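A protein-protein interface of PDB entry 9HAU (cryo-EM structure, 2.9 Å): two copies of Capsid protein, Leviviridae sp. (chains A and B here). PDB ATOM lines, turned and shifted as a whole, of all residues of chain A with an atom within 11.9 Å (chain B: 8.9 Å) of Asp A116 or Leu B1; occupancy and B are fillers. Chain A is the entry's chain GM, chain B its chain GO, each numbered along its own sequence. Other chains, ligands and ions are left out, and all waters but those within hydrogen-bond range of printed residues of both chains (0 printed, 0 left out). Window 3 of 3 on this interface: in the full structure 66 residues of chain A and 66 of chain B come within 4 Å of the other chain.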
ATOM      1  N   GLY A  97     -23.550   8.721  16.660  1.00  0.00           N
ATOM      2  CA  GLY A  97     -22.799   9.960  16.740  1.00  0.00           C
ATOM      3  C   GLY A  97     -23.660  11.201  16.781  1.00  0.00           C
ATOM      4  O   GLY A  97     -23.250  12.221  17.341  1.00  0.00           O
ATOM      5  N   SER A 100     -24.946  11.766  20.587  1.00  0.00           N
ATOM      6  CA  SER A 100     -23.948  11.784  21.640  1.00  0.00           C
ATOM      7  C   SER A 100     -23.881  13.169  22.278  1.00  0.00           C
ATOM      8  O   SER A 100     -24.576  14.104  21.875  1.00  0.00           O
ATOM      9  CB  SER A 100     -22.587  11.368  21.085  1.00  0.00           C
ATOM     10  OG  SER A 100     -22.276  12.094  19.908  1.00  0.00           O
ATOM     11  N   SER A 101     -23.030  13.301  23.298  1.00  0.00           N
ATOM     12  CA  SER A 101     -22.797  14.603  23.908  1.00  0.00           C
ATOM     13  C   SER A 101     -22.115  15.570  22.951  1.00  0.00           C
ATOM     14  O   SER A 101     -22.143  16.782  23.188  1.00  0.00           O
ATOM     15  CB  SER A 101     -21.959  14.446  25.175  1.00  0.00           C
ATOM     16  OG  SER A 101     -20.682  13.914  24.873  1.00  0.00           O
ATOM     17  N   VAL A 102     -21.497  15.060  21.884  1.00  0.00           N
ATOM     18  CA  VAL A 102     -20.887  15.930  20.884  1.00  0.00           C
ATOM     19  C   VAL A 102     -21.946  16.808  20.230  1.00  0.00           C
ATOM     20  O   VAL A 102     -21.746  18.013  20.039  1.00  0.00           O
ATOM     21  CB  VAL A 102     -20.124  15.088  19.844  1.00  0.00           C
ATOM     22  CG1 VAL A 102     -19.634  15.959  18.699  1.00  0.00           C
ATOM     23  CG2 VAL A 102     -18.966  14.357  20.502  1.00  0.00           C
ATOM     24  N   ASP A 105     -23.156  19.416  22.836  1.00  0.00           N
ATOM     25  CA  ASP A 105     -22.207  20.499  23.076  1.00  0.00           C
ATOM     26  C   ASP A 105     -22.139  21.451  21.890  1.00  0.00           C
ATOM     27  O   ASP A 105     -21.974  22.662  22.071  1.00  0.00           O
ATOM     28  CB  ASP A 105     -20.825  19.927  23.381  1.00  0.00           C
ATOM     29  CG  ASP A 105     -20.710  19.414  24.796  1.00  0.00           C
ATOM     30  OD1 ASP A 105     -19.944  18.453  25.020  1.00  0.00           O
ATOM     31  OD2 ASP A 105     -21.386  19.969  25.686  1.00  0.00           O
ATOM     32  N   VAL A 111     -19.306  23.892  20.417  1.00  0.00           N
ATOM     33  CA  VAL A 111     -18.031  23.198  20.565  1.00  0.00           C
ATOM     34  C   VAL A 111     -17.780  22.346  19.326  1.00  0.00           C
ATOM     35  O   VAL A 111     -18.562  21.443  19.011  1.00  0.00           O
ATOM     36  CB  VAL A 111     -18.015  22.339  21.837  1.00  0.00           C
ATOM     37  CG1 VAL A 111     -16.755  21.491  21.888  1.00  0.00           C
ATOM     38  CG2 VAL A 111     -18.120  23.220  23.067  1.00  0.00           C
ATOM     39  N   ILE A 112     -16.681  22.629  18.628  1.00  0.00           N
ATOM     40  CA  ILE A 112     -16.287  21.888  17.435  1.00  0.00           C
ATOM     41  C   ILE A 112     -15.006  21.097  17.640  1.00  0.00           C
ATOM     42  O   ILE A 112     -14.545  20.434  16.700  1.00  0.00           O
ATOM     43  CB  ILE A 112     -16.149  22.821  16.218  1.00  0.00           C
ATOM     44  CG1 ILE A 112     -15.132  23.927  16.502  1.00  0.00           C
ATOM     45  CG2 ILE A 112     -17.496  23.416  15.843  1.00  0.00           C
ATOM     46  CD1 ILE A 112     -14.908  24.859  15.340  1.00  0.00           C
ATOM     47  N   HIS A 113     -14.414  21.144  18.831  1.00  0.00           N
ATOM     48  CA  HIS A 113     -13.215  20.383  19.166  1.00  0.00           C
ATOM     49  C   HIS A 113     -13.589  19.344  20.217  1.00  0.00           C
ATOM     50  O   HIS A 113     -13.880  19.700  21.364  1.00  0.00           O
ATOM     51  CB  HIS A 113     -12.110  21.300  19.687  1.00  0.00           C
ATOM     52  CG  HIS A 113     -11.827  22.479  18.808  1.00  0.00           C
ATOM     53  ND1 HIS A 113     -10.996  22.409  17.712  1.00  0.00           N
ATOM     54  CD2 HIS A 113     -12.257  23.761  18.872  1.00  0.00           C
ATOM     55  CE1 HIS A 113     -10.930  23.595  17.135  1.00  0.00           C
ATOM     56  NE2 HIS A 113     -11.688  24.433  17.818  1.00  0.00           N
ATOM     57  N   LEU A 114     -13.582  18.064  19.840  1.00  0.00           N
ATOM     58  CA  LEU A 114     -13.912  16.994  20.784  1.00  0.00           C
ATOM     59  C   LEU A 114     -12.624  16.382  21.331  1.00  0.00           C
ATOM     60  O   LEU A 114     -12.259  15.246  21.034  1.00  0.00           O
ATOM     61  CB  LEU A 114     -14.826  15.938  20.149  1.00  0.00           C
ATOM     62  CG  LEU A 114     -14.780  15.368  18.722  1.00  0.00           C
ATOM     63  CD1 LEU A 114     -15.317  16.370  17.743  1.00  0.00           C
ATOM     64  CD2 LEU A 114     -13.406  14.894  18.283  1.00  0.00           C
ATOM     65  N   SER A 115     -11.947  17.147  22.174  1.00  0.00           N
ATOM     66  CA  SER A 115     -10.795  16.640  22.901  1.00  0.00           C
ATOM     67  C   SER A 115     -11.252  15.931  24.175  1.00  0.00           C
ATOM     68  O   SER A 115     -12.276  16.274  24.769  1.00  0.00           O
ATOM     69  CB  SER A 115      -9.832  17.780  23.241  1.00  0.00           C
ATOM     70  OG  SER A 115     -10.298  18.531  24.349  1.00  0.00           O
ATOM     71  N   ASP A 116     -10.482  14.927  24.590  1.00  0.00           N
ATOM     72  CA  ASP A 116      -9.318  14.357  23.919  1.00  0.00           C
ATOM     73  C   ASP A 116      -9.364  12.833  23.986  1.00  0.00           C
ATOM     74  O   ASP A 116      -8.596  12.147  23.314  1.00  0.00           O
ATOM     75  CB  ASP A 116      -8.023  14.882  24.546  1.00  0.00           C
ATOM     76  CG  ASP A 116      -6.802  14.593  23.696  1.00  0.00           C
ATOM     77  OD1 ASP A 116      -6.263  13.470  23.784  1.00  0.00           O
ATOM     78  OD2 ASP A 116      -6.382  15.489  22.936  1.00  0.00           O
ATOM     79  N   ALA A 117     -10.275  12.313  24.804  1.00  0.00           N
ATOM     80  CA  ALA A 117     -10.404  10.874  25.005  1.00  0.00           C
ATOM     81  C   ALA A 117     -10.761  10.152  23.709  1.00  0.00           C
ATOM     82  O   ALA A 117     -10.275   9.052  23.445  1.00  0.00           O
ATOM     83  CB  ALA A 117     -11.446  10.583  26.072  1.00  0.00           C
ATOM     84  OXT ALA A 117     -11.538  10.649  22.895  1.00  0.00           O
ATOM     85  N   LEU B   1      -9.902  10.264  20.442  1.00  0.00           N
ATOM     86  CA  LEU B   1     -10.850  11.067  19.682  1.00  0.00           C
ATOM     87  C   LEU B   1     -11.897  10.181  19.023  1.00  0.00           C
ATOM     88  O   LEU B   1     -11.600   9.446  18.082  1.00  0.00           O
ATOM     89  CB  LEU B   1     -10.126  11.899  18.624  1.00  0.00           C
ATOM     90  CG  LEU B   1     -10.059  13.406  18.863  1.00  0.00           C
ATOM     91  CD1 LEU B   1      -9.508  13.707  20.242  1.00  0.00           C
ATOM     92  CD2 LEU B   1      -9.215  14.071  17.791  1.00  0.00           C
ATOM     93  N   SER B   2     -13.128  10.253  19.523  1.00  0.00           N
ATOM     94  CA  SER B   2     -14.212   9.431  19.015  1.00  0.00           C
ATOM     95  C   SER B   2     -15.491  10.252  18.946  1.00  0.00           C
ATOM     96  O   SER B   2     -15.756  11.094  19.808  1.00  0.00           O
ATOM     97  CB  SER B   2     -14.435   8.191  19.890  1.00  0.00           C
ATOM     98  OG  SER B   2     -15.721   7.640  19.677  1.00  0.00           O
ATOM     99  N   ILE B   3     -16.275  10.002  17.905  1.00  0.00           N
ATOM    100  CA  ILE B   3     -17.604  10.578  17.751  1.00  0.00           C
ATOM    101  C   ILE B   3     -18.583   9.416  17.729  1.00  0.00           C
ATOM    102  O   ILE B   3     -18.573   8.603  16.797  1.00  0.00           O
ATOM    103  CB  ILE B   3     -17.724  11.430  16.481  1.00  0.00           C
ATOM    104  CG1 ILE B   3     -16.871  12.692  16.610  1.00  0.00           C
ATOM    105  CG2 ILE B   3     -19.177  11.787  16.219  1.00  0.00           C
ATOM    106  CD1 ILE B   3     -16.853  13.548  15.367  1.00  0.00           C
ATOM    107  N   GLY B   4     -19.429   9.333  18.752  1.00  0.00           N
ATOM    108  CA  GLY B   4     -20.295   8.182  18.908  1.00  0.00           C
ATOM    109  C   GLY B   4     -19.494   6.923  19.157  1.00  0.00           C
ATOM    110  O   GLY B   4     -18.728   6.848  20.123  1.00  0.00           O
ATOM    111  N   THR B   5     -19.660   5.923  18.295  1.00  0.00           N
ATOM    112  CA  THR B   5     -18.887   4.693  18.378  1.00  0.00           C
ATOM    113  C   THR B   5     -17.735   4.651  17.385  1.00  0.00           C
ATOM    114  O   THR B   5     -17.016   3.649  17.334  1.00  0.00           O
ATOM    115  CB  THR B   5     -19.798   3.480  18.159  1.00  0.00           C
ATOM    116  OG1 THR B   5     -20.378   3.541  16.851  1.00  0.00           O
ATOM    117  CG2 THR B   5     -20.908   3.455  19.200  1.00  0.00           C
ATOM    118  N   LYS B   6     -17.534   5.710  16.605  1.00  0.00           N
ATOM    119  CA  LYS B   6     -16.519   5.736  15.560  1.00  0.00           C
ATOM    120  C   LYS B   6     -15.308   6.529  16.035  1.00  0.00           C
ATOM    121  O   LYS B   6     -15.441   7.685  16.448  1.00  0.00           O
ATOM    122  CB  LYS B   6     -17.079   6.344  14.276  1.00  0.00           C
ATOM    123  CG  LYS B   6     -16.099   6.342  13.116  1.00  0.00           C
ATOM    124  CD  LYS B   6     -16.818   6.460  11.784  1.00  0.00           C
ATOM    125  CE  LYS B   6     -17.328   7.872  11.557  1.00  0.00           C
ATOM    126  NZ  LYS B   6     -16.468   8.619  10.599  1.00  0.00           N
ATOM    127  N   ASN B   7     -14.135   5.906  15.973  1.00  0.00           N
ATOM    128  CA  ASN B   7     -12.894   6.624  16.224  1.00  0.00           C
ATOM    129  C   ASN B   7     -12.536   7.481  15.018  1.00  0.00           C
ATOM    130  O   ASN B   7     -12.567   7.020  13.875  1.00  0.00           O
ATOM    131  CB  ASN B   7     -11.760   5.646  16.529  1.00  0.00           C
ATOM    132  CG  ASN B   7     -12.023   4.816  17.767  1.00  0.00           C
ATOM    133  OD1 ASN B   7     -13.102   4.881  18.356  1.00  0.00           O
ATOM    134  ND2 ASN B   7     -11.033   4.030  18.172  1.00  0.00           N
ATOM    135  N   VAL B   8     -12.191   8.741  15.277  1.00  0.00           N
ATOM    136  CA  VAL B   8     -11.867   9.695  14.228  1.00  0.00           C
ATOM    137  C   VAL B   8     -10.563  10.395  14.584  1.00  0.00           C
ATOM    138  O   VAL B   8     -10.062  10.300  15.704  1.00  0.00           O
ATOM    139  CB  VAL B   8     -12.992  10.729  14.005  1.00  0.00           C
ATOM    140  CG1 VAL B   8     -14.164  10.093  13.270  1.00  0.00           C
ATOM    141  CG2 VAL B   8     -13.439  11.319  15.332  1.00  0.00           C
ATOM    142  N   SER B   9     -10.015  11.100  13.601  1.00  0.00           N
ATOM    143  CA  SER B   9      -8.831  11.920  13.786  1.00  0.00           C
ATOM    144  C   SER B   9      -9.051  13.263  13.109  1.00  0.00           C
ATOM    145  O   SER B   9      -9.846  13.388  12.176  1.00  0.00           O
ATOM    146  CB  SER B   9      -7.576  11.239  13.223  1.00  0.00           C
ATOM    147  OG  SER B   9      -7.571  11.266  11.806  1.00  0.00           O
ATOM    148  N   ILE B  10      -8.338  14.278  13.596  1.00  0.00           N
ATOM    149  CA  ILE B  10      -8.449  15.609  13.016  1.00  0.00           C
ATOM    150  C   ILE B  10      -7.890  15.587  11.601  1.00  0.00           C
ATOM    151  O   ILE B  10      -6.755  15.153  11.369  1.00  0.00           O
ATOM    152  CB  ILE B  10      -7.725  16.645  13.889  1.00  0.00           C
ATOM    153  CG1 ILE B  10      -8.328  16.674  15.291  1.00  0.00           C
ATOM    154  CG2 ILE B  10      -7.800  18.023  13.252  1.00  0.00           C
ATOM    155  CD1 ILE B  10      -7.328  16.985  16.379  1.00  0.00           C
ATOM    156  N   TYR B  11      -8.690  16.054  10.647  1.00  0.00           N
ATOM    157  CA  TYR B  11      -8.319  16.070   9.241  1.00  0.00           C
ATOM    158  C   TYR B  11      -8.080  17.479   8.720  1.00  0.00           C
ATOM    159  O   TYR B  11      -7.043  17.745   8.106  1.00  0.00           O
ATOM    160  CB  TYR B  11      -9.410  15.381   8.410  1.00  0.00           C
ATOM    161  CG  TYR B  11      -9.143  15.366   6.923  1.00  0.00           C
ATOM    162  CD1 TYR B  11      -8.058  14.674   6.403  1.00  0.00           C
ATOM    163  CD2 TYR B  11      -9.976  16.035   6.040  1.00  0.00           C
ATOM    164  CE1 TYR B  11      -7.811  14.650   5.048  1.00  0.00           C
ATOM    165  CE2 TYR B  11      -9.736  16.018   4.681  1.00  0.00           C
ATOM    166  CZ  TYR B  11      -8.651  15.323   4.192  1.00  0.00           C
ATOM    167  OH  TYR B  11      -8.403  15.300   2.840  1.00  0.00           O
ATOM    168  N   VAL B  18     -14.217  22.135  11.988  1.00  0.00           N
ATOM    169  CA  VAL B  18     -13.197  21.103  12.115  1.00  0.00           C
ATOM    170  C   VAL B  18     -13.725  19.849  11.438  1.00  0.00           C
ATOM    171  O   VAL B  18     -14.761  19.308  11.844  1.00  0.00           O
ATOM    172  CB  VAL B  18     -12.832  20.821  13.580  1.00  0.00           C
ATOM    173  CG1 VAL B  18     -11.653  19.864  13.649  1.00  0.00           C
ATOM    174  CG2 VAL B  18     -12.519  22.112  14.313  1.00  0.00           C
ATOM    175  N   ILE B  19     -13.018  19.388  10.415  1.00  0.00           N
ATOM    176  CA  ILE B  19     -13.380  18.165   9.710  1.00  0.00           C
ATOM    177  C   ILE B  19     -12.584  17.017  10.313  1.00  0.00           C
ATOM    178  O   ILE B  19     -11.359  17.098  10.440  1.00  0.00           O
ATOM    179  CB  ILE B  19     -13.117  18.289   8.203  1.00  0.00           C
ATOM    180  CG1 ILE B  19     -13.718  19.588   7.664  1.00  0.00           C
ATOM    181  CG2 ILE B  19     -13.683  17.088   7.462  1.00  0.00           C
ATOM    182  CD1 ILE B  19     -13.444  19.822   6.203  1.00  0.00           C
ATOM    183  N   TYR B  20     -13.280  15.954  10.696  1.00  0.00           N
ATOM    184  CA  TYR B  20     -12.654  14.751  11.214  1.00  0.00           C
ATOM    185  C   TYR B  20     -12.783  13.633  10.191  1.00  0.00           C
ATOM    186  O   TYR B  20     -13.725  13.604   9.397  1.00  0.00           O
ATOM    187  CB  TYR B  20     -13.280  14.330  12.546  1.00  0.00           C
ATOM    188  CG  TYR B  20     -13.174  15.393  13.612  1.00  0.00           C
ATOM    189  CD1 TYR B  20     -14.143  16.379  13.733  1.00  0.00           C
ATOM    190  CD2 TYR B  20     -12.096  15.424  14.482  1.00  0.00           C
ATOM    191  CE1 TYR B  20     -14.044  17.357  14.695  1.00  0.00           C
ATOM    192  CE2 TYR B  20     -11.989  16.398  15.449  1.00  0.00           C
ATOM    193  CZ  TYR B  20     -12.966  17.362  15.552  1.00  0.00           C
ATOM    194  OH  TYR B  20     -12.867  18.337  16.514  1.00  0.00           O
ATOM    195  N   ALA B  21     -11.820  12.720  10.206  1.00  0.00           N
ATOM    196  CA  ALA B  21     -11.743  11.647   9.227  1.00  0.00           C
ATOM    197  C   ALA B  21     -11.934  10.306   9.917  1.00  0.00           C
ATOM    198  O   ALA B  21     -11.349  10.057  10.976  1.00  0.00           O
ATOM    199  CB  ALA B  21     -10.403  11.675   8.489  1.00  0.00           C
ATOM    200  N   GLY B  22     -12.751   9.447   9.315  1.00  0.00           N
ATOM    201  CA  GLY B  22     -12.926   8.101   9.800  1.00  0.00           C
ATOM    202  C   GLY B  22     -11.707   7.255   9.503  1.00  0.00           C
ATOM    203  O   GLY B  22     -10.797   7.671   8.779  1.00  0.00           O
ATOM    204  N   PRO B  23     -11.660   6.047  10.069  1.00  0.00           N
ATOM    205  CA  PRO B  23     -10.496   5.179   9.828  1.00  0.00           C
ATOM    206  C   PRO B  23     -10.304   4.829   8.363  1.00  0.00           C
ATOM    207  O   PRO B  23      -9.163   4.646   7.923  1.00  0.00           O
ATOM    208  CB  PRO B  23     -10.799   3.933  10.674  1.00  0.00           C
ATOM    209  CG  PRO B  23     -11.970   4.295  11.543  1.00  0.00           C
ATOM    210  CD  PRO B  23     -12.717   5.366  10.830  1.00  0.00           C
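The backbone carbonyl oxygen of Ile A112 is in hydrogen-bond range of the side-chain hydroxyl of Tyr B20, at 2.7 Å.
The backbone NH (N) of Leu A114 sits close to the side-chain hydroxyl (OH) of Tyr B20 (3.4 Å).
The chain-end carboxylate (OXT) of Ala A117 is in hydrogen-bond range of the backbone NH (N) of Leu B1, at 3.0 Å.
The backbone carbonyl oxygen (O) of Gly A97 lies within hydrogen-bond range of the side-chain hydroxyl (OG) of Ser A100 (2.7 Å).
The backbone NH (N) of Val B8 lies within hydrogen-bond range of the backbone carbonyl oxygen (O) of Leu B1 (3.0 Å).
O of Gly B4 sits at hydrogen-bond distance from OG of Ser B2, 3.1 Å away.
The side-chain hydroxyl of Ser B2 is in hydrogen-bond range of the backbone carbonyl oxygen of Lys B6 (3.2 Å).
Gly B4 touches Gly A97.
Ile A112 touches Val B18.
CE1 of His A113 touches CG2 of Val B18 (3.6 Å).
Tyr B20 touches His A113.
Leu A114 touches Leu B1 (O to CD1, 3.3 Å).
Leu A114 touches Ile B3 (CD1 to CD1, 3.996 Å).
Asp A116 touches Leu B1.
OXT of Ala A117 touches N of Ser B2, at 3.7 Å.
Printed residues of chain B within 4 Å of Gly A97: Gly B4 (3.8 Å).
Of the printed residues of chain B, Ile A112 touches Val B18 and Tyr B20.
Printed residues of chain B within 4 Å of His A113: Val B18 (3.6 Å) and Tyr B20 (3.4 Å).
Of the printed residues of chain B, Leu A114 touches Leu B1, Ile B3 and Tyr B20.
No residue of chain B comes within 4 Å of Ser A115.
Asp A116 touches one residue of chain B.
Ala A117 touches just these residues of chain B: Leu B1 (3.0 Å) and Ser B2 (3.7 Å).
Leu B1 touches just these residues of chain A: Leu A114 (3.3 Å), Asp A116 (3.6 Å) and Ala A117 (3.0 Å).
Ser B2 touches just one residue of chain A: Ala A117 (3.7 Å).
No residue of chain A comes within 4 Å of Asn B7.
No residue of chain A comes within 4 Å of Ile B10.
Pro B23 touches none of the printed residues of chain A.
The nearest residue of chain B that does not touch Asp A116 is Ser B2 (6.2 Å).
Hydrophobic or aromatic side chains of chain A that line the printed part of chain B: Ile A112, His A113 and Leu A114.
Printed residues of chain B that touch a printed residue of chain A: Leu B1, Ser B2, Ile B3, Gly B4, Val B18 and Tyr B20.
Hydrophobic or aromatic side chains of chain B that line the printed part of chain A: Leu B1, Ile B3, Val B18 and Tyr B20.
Among the printed residues, no Asp or Glu carboxylate lies within 4 Å of a Lys or Arg side-chain nitrogen of the other chain.
No position is printed for both chains.
Of the 11 pairs that touch across the chains among the printed residues, none has its exchanged pair printed and touching as well.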
